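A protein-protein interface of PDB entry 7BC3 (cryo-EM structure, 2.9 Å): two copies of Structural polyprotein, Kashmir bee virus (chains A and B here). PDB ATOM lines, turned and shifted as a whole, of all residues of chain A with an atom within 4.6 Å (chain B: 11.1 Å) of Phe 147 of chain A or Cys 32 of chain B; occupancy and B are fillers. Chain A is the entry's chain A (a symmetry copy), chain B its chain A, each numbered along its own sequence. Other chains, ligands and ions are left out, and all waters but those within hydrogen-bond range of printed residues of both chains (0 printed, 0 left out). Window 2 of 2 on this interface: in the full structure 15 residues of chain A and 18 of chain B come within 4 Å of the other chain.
O of Gly 31 of chain B lies close to O of Phe 147 of chain A (2.4 Å). The backbone carbonyl oxygen of Gly 31 of chain B lies within hydrogen-bond range of the backbone NH of Ser 149 of chain A, 3.0 Å away. The side-chain hydroxyl of Tyr 148 of chain A lies close to the side-chain carboxylate of Glu 34 of chain B, at 2.3 Å. NH1 of Arg 30 of chain B lies close to NH2 of Arg 152 of chain A.
The side-chain carboxylate of Glu 26 of chain B is in salt-bridge range of the guanidinium group of Arg 30 of chain B (3.0 Å). SG of Cys 32 of chain B sits at hydrogen-bond distance from O of Glu 34 of chain B (3.3 Å). The backbone carbonyl oxygen (O) of Tyr 151 of chain A lies within hydrogen-bond range of the side-chain hydroxyl (OG) of Ser 149 of chain A (2.5 Å).
NH2 of Arg 89 of chain A touches O of Met 29 of chain B (3.98 Å). Phe 147 of chain A touches Arg 30 of chain B. Cys 32 of chain B touches Phe 147 of chain A. Gly 31 of chain B touches Tyr 148 of chain A. Cys 32 of chain B touches Tyr 148 of chain A (O to CE1, 3.7 Å).
Phe 147 of chain A touches just these residues of chain B: Arg 30, Gly 31 and Cys 32. Cys 32 of chain B touches just these residues of chain A: Phe 147 and Tyr 148. No residue of chain B comes within 4 Å of Gly 90 of chain A. No residue of chain B comes within 4 Å of Gly 91 of chain A. No residue of chain B comes within 4 Å of Pro 146 of chain A. No residue of chain B comes within 4 Å of Ile 154 of chain A. Printed residues of chain A within 4 Å of Glu 34 of chain B: Tyr 148 (2.3 Å). Of the printed residues of chain A, Gly 31 of chain B touches Phe 147, Tyr 148 and Ser 149. Of the printed residues of chain B, Arg 89 of chain A touches Met 29 (3.98 Å). Ser 25 of chain B touches none of the printed residues of chain A. Met 23 of chain B touches none of the printed residues of chain A. The nearest printed residue of chain A that does not touch Cys 32 of chain B is Pro 146 of chain A (4.8 Å). The nearest printed residue of chain B that does not touch Arg 152 of chain A is Gly 31 of chain B (5.4 Å).
Of the 12 printed residues of chain A, 5 touch a printed residue of chain B. Of the 15 printed residues of chain B, 5 touch a printed residue of chain A. Among the printed residues, 9 pairs touch across the chains. Among the printed residues, no Asp or Glu carboxylate lies within 4 Å of a Lys or Arg side-chain nitrogen of the other chain.
No position is printed for both chains.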
ATOM      1  N   ARG A  89      15.381  16.558  21.650  1.00  0.00           N
ATOM      2  CA  ARG A  89      15.236  15.152  21.327  1.00  0.00           C
ATOM      3  C   ARG A  89      15.312  14.359  22.621  1.00  0.00           C
ATOM      4  O   ARG A  89      15.555  14.908  23.696  1.00  0.00           O
ATOM      5  CB  ARG A  89      16.320  14.674  20.363  1.00  0.00           C
ATOM      6  CG  ARG A  89      17.599  14.308  21.074  1.00  0.00           C
ATOM      7  CD  ARG A  89      18.756  14.227  20.133  1.00  0.00           C
ATOM      8  NE  ARG A  89      18.716  13.016  19.321  1.00  0.00           N
ATOM      9  CZ  ARG A  89      19.341  11.886  19.634  1.00  0.00           C
ATOM     10  NH1 ARG A  89      20.047  11.784  20.751  1.00  0.00           N
ATOM     11  NH2 ARG A  89      19.251  10.843  18.825  1.00  0.00           N
ATOM     12  N   GLY A  90      15.114  13.056  22.508  1.00  0.00           N
ATOM     13  CA  GLY A  90      15.294  12.175  23.639  1.00  0.00           C
ATOM     14  C   GLY A  90      14.062  12.072  24.509  1.00  0.00           C
ATOM     15  O   GLY A  90      13.043  12.741  24.312  1.00  0.00           O
ATOM     16  N   GLY A  91      14.174  11.200  25.509  1.00  0.00           N
ATOM     17  CA  GLY A  91      13.087  10.922  26.417  1.00  0.00           C
ATOM     18  C   GLY A  91      13.166  11.742  27.692  1.00  0.00           C
ATOM     19  O   GLY A  91      14.052  12.570  27.893  1.00  0.00           O
ATOM     20  N   VAL A 145      10.004   7.849  29.996  1.00  0.00           N
ATOM     21  CA  VAL A 145       9.321   7.858  28.708  1.00  0.00           C
ATOM     22  C   VAL A 145      10.386   7.885  27.617  1.00  0.00           C
ATOM     23  O   VAL A 145      11.185   8.830  27.570  1.00  0.00           O
ATOM     24  CB  VAL A 145       8.373   9.058  28.576  1.00  0.00           C
ATOM     25  CG1 VAL A 145       7.653   9.011  27.246  1.00  0.00           C
ATOM     26  CG2 VAL A 145       7.380   9.078  29.720  1.00  0.00           C
ATOM     27  N   PRO A 146      10.443   6.899  26.732  1.00  0.00           N
ATOM     28  CA  PRO A 146      11.447   6.909  25.667  1.00  0.00           C
ATOM     29  C   PRO A 146      11.091   7.929  24.590  1.00  0.00           C
ATOM     30  O   PRO A 146      10.072   8.614  24.651  1.00  0.00           O
ATOM     31  CB  PRO A 146      11.401   5.481  25.115  1.00  0.00           C
ATOM     32  CG  PRO A 146      10.646   4.691  26.109  1.00  0.00           C
ATOM     33  CD  PRO A 146       9.691   5.636  26.732  1.00  0.00           C
ATOM     34  N   PHE A 147      11.962   8.014  23.591  1.00  0.00           N
ATOM     35  CA  PHE A 147      11.759   8.905  22.455  1.00  0.00           C
ATOM     36  C   PHE A 147      11.166   8.116  21.291  1.00  0.00           C
ATOM     37  O   PHE A 147      11.836   7.768  20.321  1.00  0.00           O
ATOM     38  CB  PHE A 147      13.073   9.573  22.069  1.00  0.00           C
ATOM     39  CG  PHE A 147      12.915  10.741  21.140  1.00  0.00           C
ATOM     40  CD1 PHE A 147      12.048  11.773  21.442  1.00  0.00           C
ATOM     41  CD2 PHE A 147      13.644  10.807  19.969  1.00  0.00           C
ATOM     42  CE1 PHE A 147      11.909  12.845  20.589  1.00  0.00           C
ATOM     43  CE2 PHE A 147      13.506  11.878  19.116  1.00  0.00           C
ATOM     44  CZ  PHE A 147      12.639  12.896  19.428  1.00  0.00           C
ATOM     45  N   TYR A 148       9.874   7.829  21.418  1.00  0.00           N
ATOM     46  CA  TYR A 148       9.118   7.158  20.364  1.00  0.00           C
ATOM     47  C   TYR A 148       8.575   8.230  19.433  1.00  0.00           C
ATOM     48  O   TYR A 148       7.521   8.812  19.686  1.00  0.00           O
ATOM     49  CB  TYR A 148       7.997   6.318  20.958  1.00  0.00           C
ATOM     50  CG  TYR A 148       8.458   5.052  21.637  1.00  0.00           C
ATOM     51  CD1 TYR A 148       9.423   4.245  21.060  1.00  0.00           C
ATOM     52  CD2 TYR A 148       7.921   4.662  22.852  1.00  0.00           C
ATOM     53  CE1 TYR A 148       9.842   3.090  21.674  1.00  0.00           C
ATOM     54  CE2 TYR A 148       8.333   3.507  23.474  1.00  0.00           C
ATOM     55  CZ  TYR A 148       9.295   2.725  22.881  1.00  0.00           C
ATOM     56  OH  TYR A 148       9.710   1.572  23.494  1.00  0.00           O
ATOM     57  N   SER A 149       9.297   8.489  18.345  1.00  0.00           N
ATOM     58  CA  SER A 149       9.033   9.643  17.504  1.00  0.00           C
ATOM     59  C   SER A 149       8.978   9.239  16.041  1.00  0.00           C
ATOM     60  O   SER A 149       9.662   8.307  15.607  1.00  0.00           O
ATOM     61  CB  SER A 149      10.110  10.714  17.687  1.00  0.00           C
ATOM     62  OG  SER A 149       9.792  11.889  16.956  1.00  0.00           O
ATOM     63  N   TYR A 151       9.915  11.651  14.146  1.00  0.00           N
ATOM     64  CA  TYR A 151      10.913  12.628  13.750  1.00  0.00           C
ATOM     65  C   TYR A 151      12.142  12.480  14.630  1.00  0.00           C
ATOM     66  O   TYR A 151      12.047  12.084  15.795  1.00  0.00           O
ATOM     67  CB  TYR A 151      10.359  14.048  13.858  1.00  0.00           C
ATOM     68  CG  TYR A 151       9.098  14.266  13.058  1.00  0.00           C
ATOM     69  CD1 TYR A 151       9.147  14.403  11.682  1.00  0.00           C
ATOM     70  CD2 TYR A 151       7.860  14.329  13.678  1.00  0.00           C
ATOM     71  CE1 TYR A 151       8.001  14.600  10.946  1.00  0.00           C
ATOM     72  CE2 TYR A 151       6.708  14.526  12.949  1.00  0.00           C
ATOM     73  CZ  TYR A 151       6.785  14.660  11.584  1.00  0.00           C
ATOM     74  OH  TYR A 151       5.640  14.856  10.851  1.00  0.00           O
ATOM     75  N   ARG A 152      13.301  12.811  14.062  1.00  0.00           N
ATOM     76  CA  ARG A 152      14.552  12.689  14.798  1.00  0.00           C
ATOM     77  C   ARG A 152      14.709  13.797  15.825  1.00  0.00           C
ATOM     78  O   ARG A 152      15.442  13.635  16.805  1.00  0.00           O
ATOM     79  CB  ARG A 152      15.731  12.706  13.829  1.00  0.00           C
ATOM     80  CG  ARG A 152      15.913  14.021  13.106  1.00  0.00           C
ATOM     81  CD  ARG A 152      17.028  13.935  12.090  1.00  0.00           C
ATOM     82  NE  ARG A 152      16.678  13.064  10.974  1.00  0.00           N
ATOM     83  CZ  ARG A 152      17.547  12.622  10.073  1.00  0.00           C
ATOM     84  NH1 ARG A 152      18.825  12.965  10.152  1.00  0.00           N
ATOM     85  NH2 ARG A 152      17.142  11.835   9.091  1.00  0.00           N
ATOM     86  N   LYS A 153      14.037  14.921  15.609  1.00  0.00           N
ATOM     87  CA  LYS A 153      14.048  16.051  16.520  1.00  0.00           C
ATOM     88  C   LYS A 153      12.621  16.550  16.688  1.00  0.00           C
ATOM     89  O   LYS A 153      11.775  16.351  15.816  1.00  0.00           O
ATOM     90  CB  LYS A 153      14.914  17.176  15.990  1.00  0.00           C
ATOM     91  CG  LYS A 153      14.394  17.718  14.685  1.00  0.00           C
ATOM     92  CD  LYS A 153      15.428  18.530  13.979  1.00  0.00           C
ATOM     93  CE  LYS A 153      16.223  17.743  12.996  1.00  0.00           C
ATOM     94  NZ  LYS A 153      17.145  18.674  12.306  1.00  0.00           N
ATOM     95  N   ILE A 154      12.372  17.206  17.814  1.00  0.00           N
ATOM     96  CA  ILE A 154      11.054  17.771  18.121  1.00  0.00           C
ATOM     97  C   ILE A 154      11.243  19.242  18.375  1.00  0.00           C
ATOM     98  O   ILE A 154      12.101  19.651  19.141  1.00  0.00           O
ATOM     99  CB  ILE A 154      10.417  17.094  19.365  1.00  0.00           C
ATOM    100  CG1 ILE A 154      10.327  15.584  19.159  1.00  0.00           C
ATOM    101  CG2 ILE A 154       9.048  17.680  19.614  1.00  0.00           C
ATOM    102  CD1 ILE A 154       9.551  15.170  17.937  1.00  0.00           C
ATOM    103  N   MET B  23      18.979   2.808   6.409  1.00  0.00           N
ATOM    104  CA  MET B  23      18.006   3.831   6.761  1.00  0.00           C
ATOM    105  C   MET B  23      17.196   3.417   7.980  1.00  0.00           C
ATOM    106  O   MET B  23      16.933   4.233   8.870  1.00  0.00           O
ATOM    107  CB  MET B  23      17.092   4.090   5.566  1.00  0.00           C
ATOM    108  CG  MET B  23      17.822   4.530   4.305  1.00  0.00           C
ATOM    109  SD  MET B  23      16.715   4.864   2.923  1.00  0.00           S
ATOM    110  CE  MET B  23      15.851   6.315   3.521  1.00  0.00           C
ATOM    111  N   ASN B  24      16.795   2.147   8.037  1.00  0.00           N
ATOM    112  CA  ASN B  24      16.006   1.661   9.160  1.00  0.00           C
ATOM    113  C   ASN B  24      16.786   1.750  10.463  1.00  0.00           C
ATOM    114  O   ASN B  24      16.247   2.178  11.489  1.00  0.00           O
ATOM    115  CB  ASN B  24      15.575   0.223   8.892  1.00  0.00           C
ATOM    116  CG  ASN B  24      14.434   0.134   7.902  1.00  0.00           C
ATOM    117  OD1 ASN B  24      13.963   1.145   7.385  1.00  0.00           O
ATOM    118  ND2 ASN B  24      13.989  -1.082   7.626  1.00  0.00           N
ATOM    119  N   SER B  25      18.055   1.349  10.442  1.00  0.00           N
ATOM    120  CA  SER B  25      18.866   1.382  11.650  1.00  0.00           C
ATOM    121  C   SER B  25      19.121   2.813  12.100  1.00  0.00           C
ATOM    122  O   SER B  25      19.104   3.105  13.300  1.00  0.00           O
ATOM    123  CB  SER B  25      20.179   0.644  11.399  1.00  0.00           C
ATOM    124  OG  SER B  25      19.958  -0.751  11.283  1.00  0.00           O
ATOM    125  N   GLU B  26      19.351   3.724  11.152  1.00  0.00           N
ATOM    126  CA  GLU B  26      19.483   5.134  11.506  1.00  0.00           C
ATOM    127  C   GLU B  26      18.203   5.654  12.150  1.00  0.00           C
ATOM    128  O   GLU B  26      18.239   6.347  13.177  1.00  0.00           O
ATOM    129  CB  GLU B  26      19.828   5.953  10.263  1.00  0.00           C
ATOM    130  CG  GLU B  26      21.135   5.567   9.599  1.00  0.00           C
ATOM    131  CD  GLU B  26      22.328   6.303  10.176  1.00  0.00           C
ATOM    132  OE1 GLU B  26      22.173   6.972  11.218  1.00  0.00           O
ATOM    133  OE2 GLU B  26      23.423   6.215   9.581  1.00  0.00           O
ATOM    134  N   ALA B  27      17.055   5.325  11.556  1.00  0.00           N
ATOM    135  CA  ALA B  27      15.785   5.791  12.094  1.00  0.00           C
ATOM    136  C   ALA B  27      15.541   5.236  13.489  1.00  0.00           C
ATOM    137  O   ALA B  27      14.982   5.922  14.349  1.00  0.00           O
ATOM    138  CB  ALA B  27      14.650   5.397  11.153  1.00  0.00           C
ATOM    139  N   LEU B  28      15.949   3.990  13.732  1.00  0.00           N
ATOM    140  CA  LEU B  28      15.817   3.427  15.071  1.00  0.00           C
ATOM    141  C   LEU B  28      16.739   4.131  16.054  1.00  0.00           C
ATOM    142  O   LEU B  28      16.334   4.446  17.179  1.00  0.00           O
ATOM    143  CB  LEU B  28      16.122   1.934  15.046  1.00  0.00           C
ATOM    144  CG  LEU B  28      15.194   1.069  14.201  1.00  0.00           C
ATOM    145  CD1 LEU B  28      15.815  -0.294  14.000  1.00  0.00           C
ATOM    146  CD2 LEU B  28      13.834   0.953  14.847  1.00  0.00           C
ATOM    147  N   MET B  29      17.984   4.382  15.649  1.00  0.00           N
ATOM    148  CA  MET B  29      18.913   5.089  16.519  1.00  0.00           C
ATOM    149  C   MET B  29      18.401   6.475  16.871  1.00  0.00           C
ATOM    150  O   MET B  29      18.708   6.996  17.948  1.00  0.00           O
ATOM    151  CB  MET B  29      20.277   5.199  15.844  1.00  0.00           C
ATOM    152  CG  MET B  29      21.077   3.915  15.833  1.00  0.00           C
ATOM    153  SD  MET B  29      21.503   3.324  17.478  1.00  0.00           S
ATOM    154  CE  MET B  29      22.350   1.809  17.050  1.00  0.00           C
ATOM    155  N   ARG B  30      17.626   7.087  15.978  1.00  0.00           N
ATOM    156  CA  ARG B  30      17.202   8.465  16.179  1.00  0.00           C
ATOM    157  C   ARG B  30      15.806   8.612  16.776  1.00  0.00           C
ATOM    158  O   ARG B  30      15.509   9.674  17.332  1.00  0.00           O
ATOM    159  CB  ARG B  30      17.246   9.224  14.851  1.00  0.00           C
ATOM    160  CG  ARG B  30      18.641   9.418  14.303  1.00  0.00           C
ATOM    161  CD  ARG B  30      18.593   9.817  12.852  1.00  0.00           C
ATOM    162  NE  ARG B  30      19.916   9.842  12.242  1.00  0.00           N
ATOM    163  CZ  ARG B  30      20.141   9.727  10.938  1.00  0.00           C
ATOM    164  NH1 ARG B  30      19.129   9.576  10.094  1.00  0.00           N
ATOM    165  NH2 ARG B  30      21.381   9.762  10.472  1.00  0.00           N
ATOM    166  N   GLY B  31      14.947   7.599  16.678  1.00  0.00           N
ATOM    167  CA  GLY B  31      13.571   7.779  17.102  1.00  0.00           C
ATOM    168  C   GLY B  31      12.884   6.621  17.797  1.00  0.00           C
ATOM    169  O   GLY B  31      11.707   6.746  18.146  1.00  0.00           O
ATOM    170  N   CYS B  32      13.559   5.489  17.985  1.00  0.00           N
ATOM    171  CA  CYS B  32      12.991   4.396  18.769  1.00  0.00           C
ATOM    172  C   CYS B  32      13.868   3.983  19.938  1.00  0.00           C
ATOM    173  O   CYS B  32      13.379   3.890  21.069  1.00  0.00           O
ATOM    174  CB  CYS B  32      12.721   3.180  17.873  1.00  0.00           C
ATOM    175  SG  CYS B  32      11.864   1.837  18.720  1.00  0.00           S
ATOM    176  N   GLY B  33      15.154   3.738  19.702  1.00  0.00           N
ATOM    177  CA  GLY B  33      16.037   3.241  20.733  1.00  0.00           C
ATOM    178  C   GLY B  33      16.055   1.737  20.894  1.00  0.00           C
ATOM    179  O   GLY B  33      16.830   1.230  21.714  1.00  0.00           O
ATOM    180  N   GLU B  34      15.235   1.007  20.145  1.00  0.00           N
ATOM    181  CA  GLU B  34      15.199  -0.445  20.224  1.00  0.00           C
ATOM    182  C   GLU B  34      14.741  -0.980  18.876  1.00  0.00           C
ATOM    183  O   GLU B  34      14.400  -0.219  17.969  1.00  0.00           O
ATOM    184  CB  GLU B  34      14.281  -0.926  21.352  1.00  0.00           C
ATOM    185  CG  GLU B  34      12.866  -0.390  21.273  1.00  0.00           C
ATOM    186  CD  GLU B  34      12.189  -0.302  22.622  1.00  0.00           C
ATOM    187  OE1 GLU B  34      12.879  -0.428  23.655  1.00  0.00           O
ATOM    188  OE2 GLU B  34      10.958  -0.107  22.649  1.00  0.00           O
ATOM    189  N   GLN B  35      14.742  -2.306  18.754  1.00  0.00           N
ATOM    190  CA  GLN B  35      14.352  -2.968  17.515  1.00  0.00           C
ATOM    191  C   GLN B  35      13.629  -4.262  17.847  1.00  0.00           C
ATOM    192  O   GLN B  35      14.202  -5.150  18.485  1.00  0.00           O
ATOM    193  CB  GLN B  35      15.567  -3.251  16.630  1.00  0.00           C
ATOM    194  CG  GLN B  35      15.214  -3.506  15.180  1.00  0.00           C
ATOM    195  CD  GLN B  35      16.427  -3.784  14.322  1.00  0.00           C
ATOM    196  OE1 GLN B  35      17.537  -3.356  14.634  1.00  0.00           O
ATOM    197  NE2 GLN B  35      16.220  -4.507  13.233  1.00  0.00           N
ATOM    198  N   ILE B  36      12.379  -4.365  17.412  1.00  0.00           N
ATOM    199  CA  ILE B  36      11.577  -5.571  17.576  1.00  0.00           C
ATOM    200  C   ILE B  36      11.647  -6.356  16.275  1.00  0.00           C
ATOM    201  O   ILE B  36      11.205  -5.875  15.226  1.00  0.00           O
ATOM    202  CB  ILE B  36      10.123  -5.237  17.943  1.00  0.00           C
ATOM    203  CG1 ILE B  36      10.076  -4.293  19.144  1.00  0.00           C
ATOM    204  CG2 ILE B  36       9.353  -6.506  18.252  1.00  0.00           C
ATOM    205  CD1 ILE B  36       8.770  -3.573  19.303  1.00  0.00           C
ATOM    206  N   VAL B  37      12.205  -7.562  16.344  1.00  0.00           N
ATOM    207  CA  VAL B  37      12.365  -8.414  15.171  1.00  0.00           C
ATOM    208  C   VAL B  37      11.619  -9.730  15.296  1.00  0.00           C
ATOM    209  O   VAL B  37      11.575 -10.492  14.319  1.00  0.00           O
ATOM    210  CB  VAL B  37      13.856  -8.683  14.875  1.00  0.00           C
ATOM    211  CG1 VAL B  37      14.603  -7.377  14.724  1.00  0.00           C
ATOM    212  CG2 VAL B  37      14.474  -9.520  15.976  1.00  0.00           C
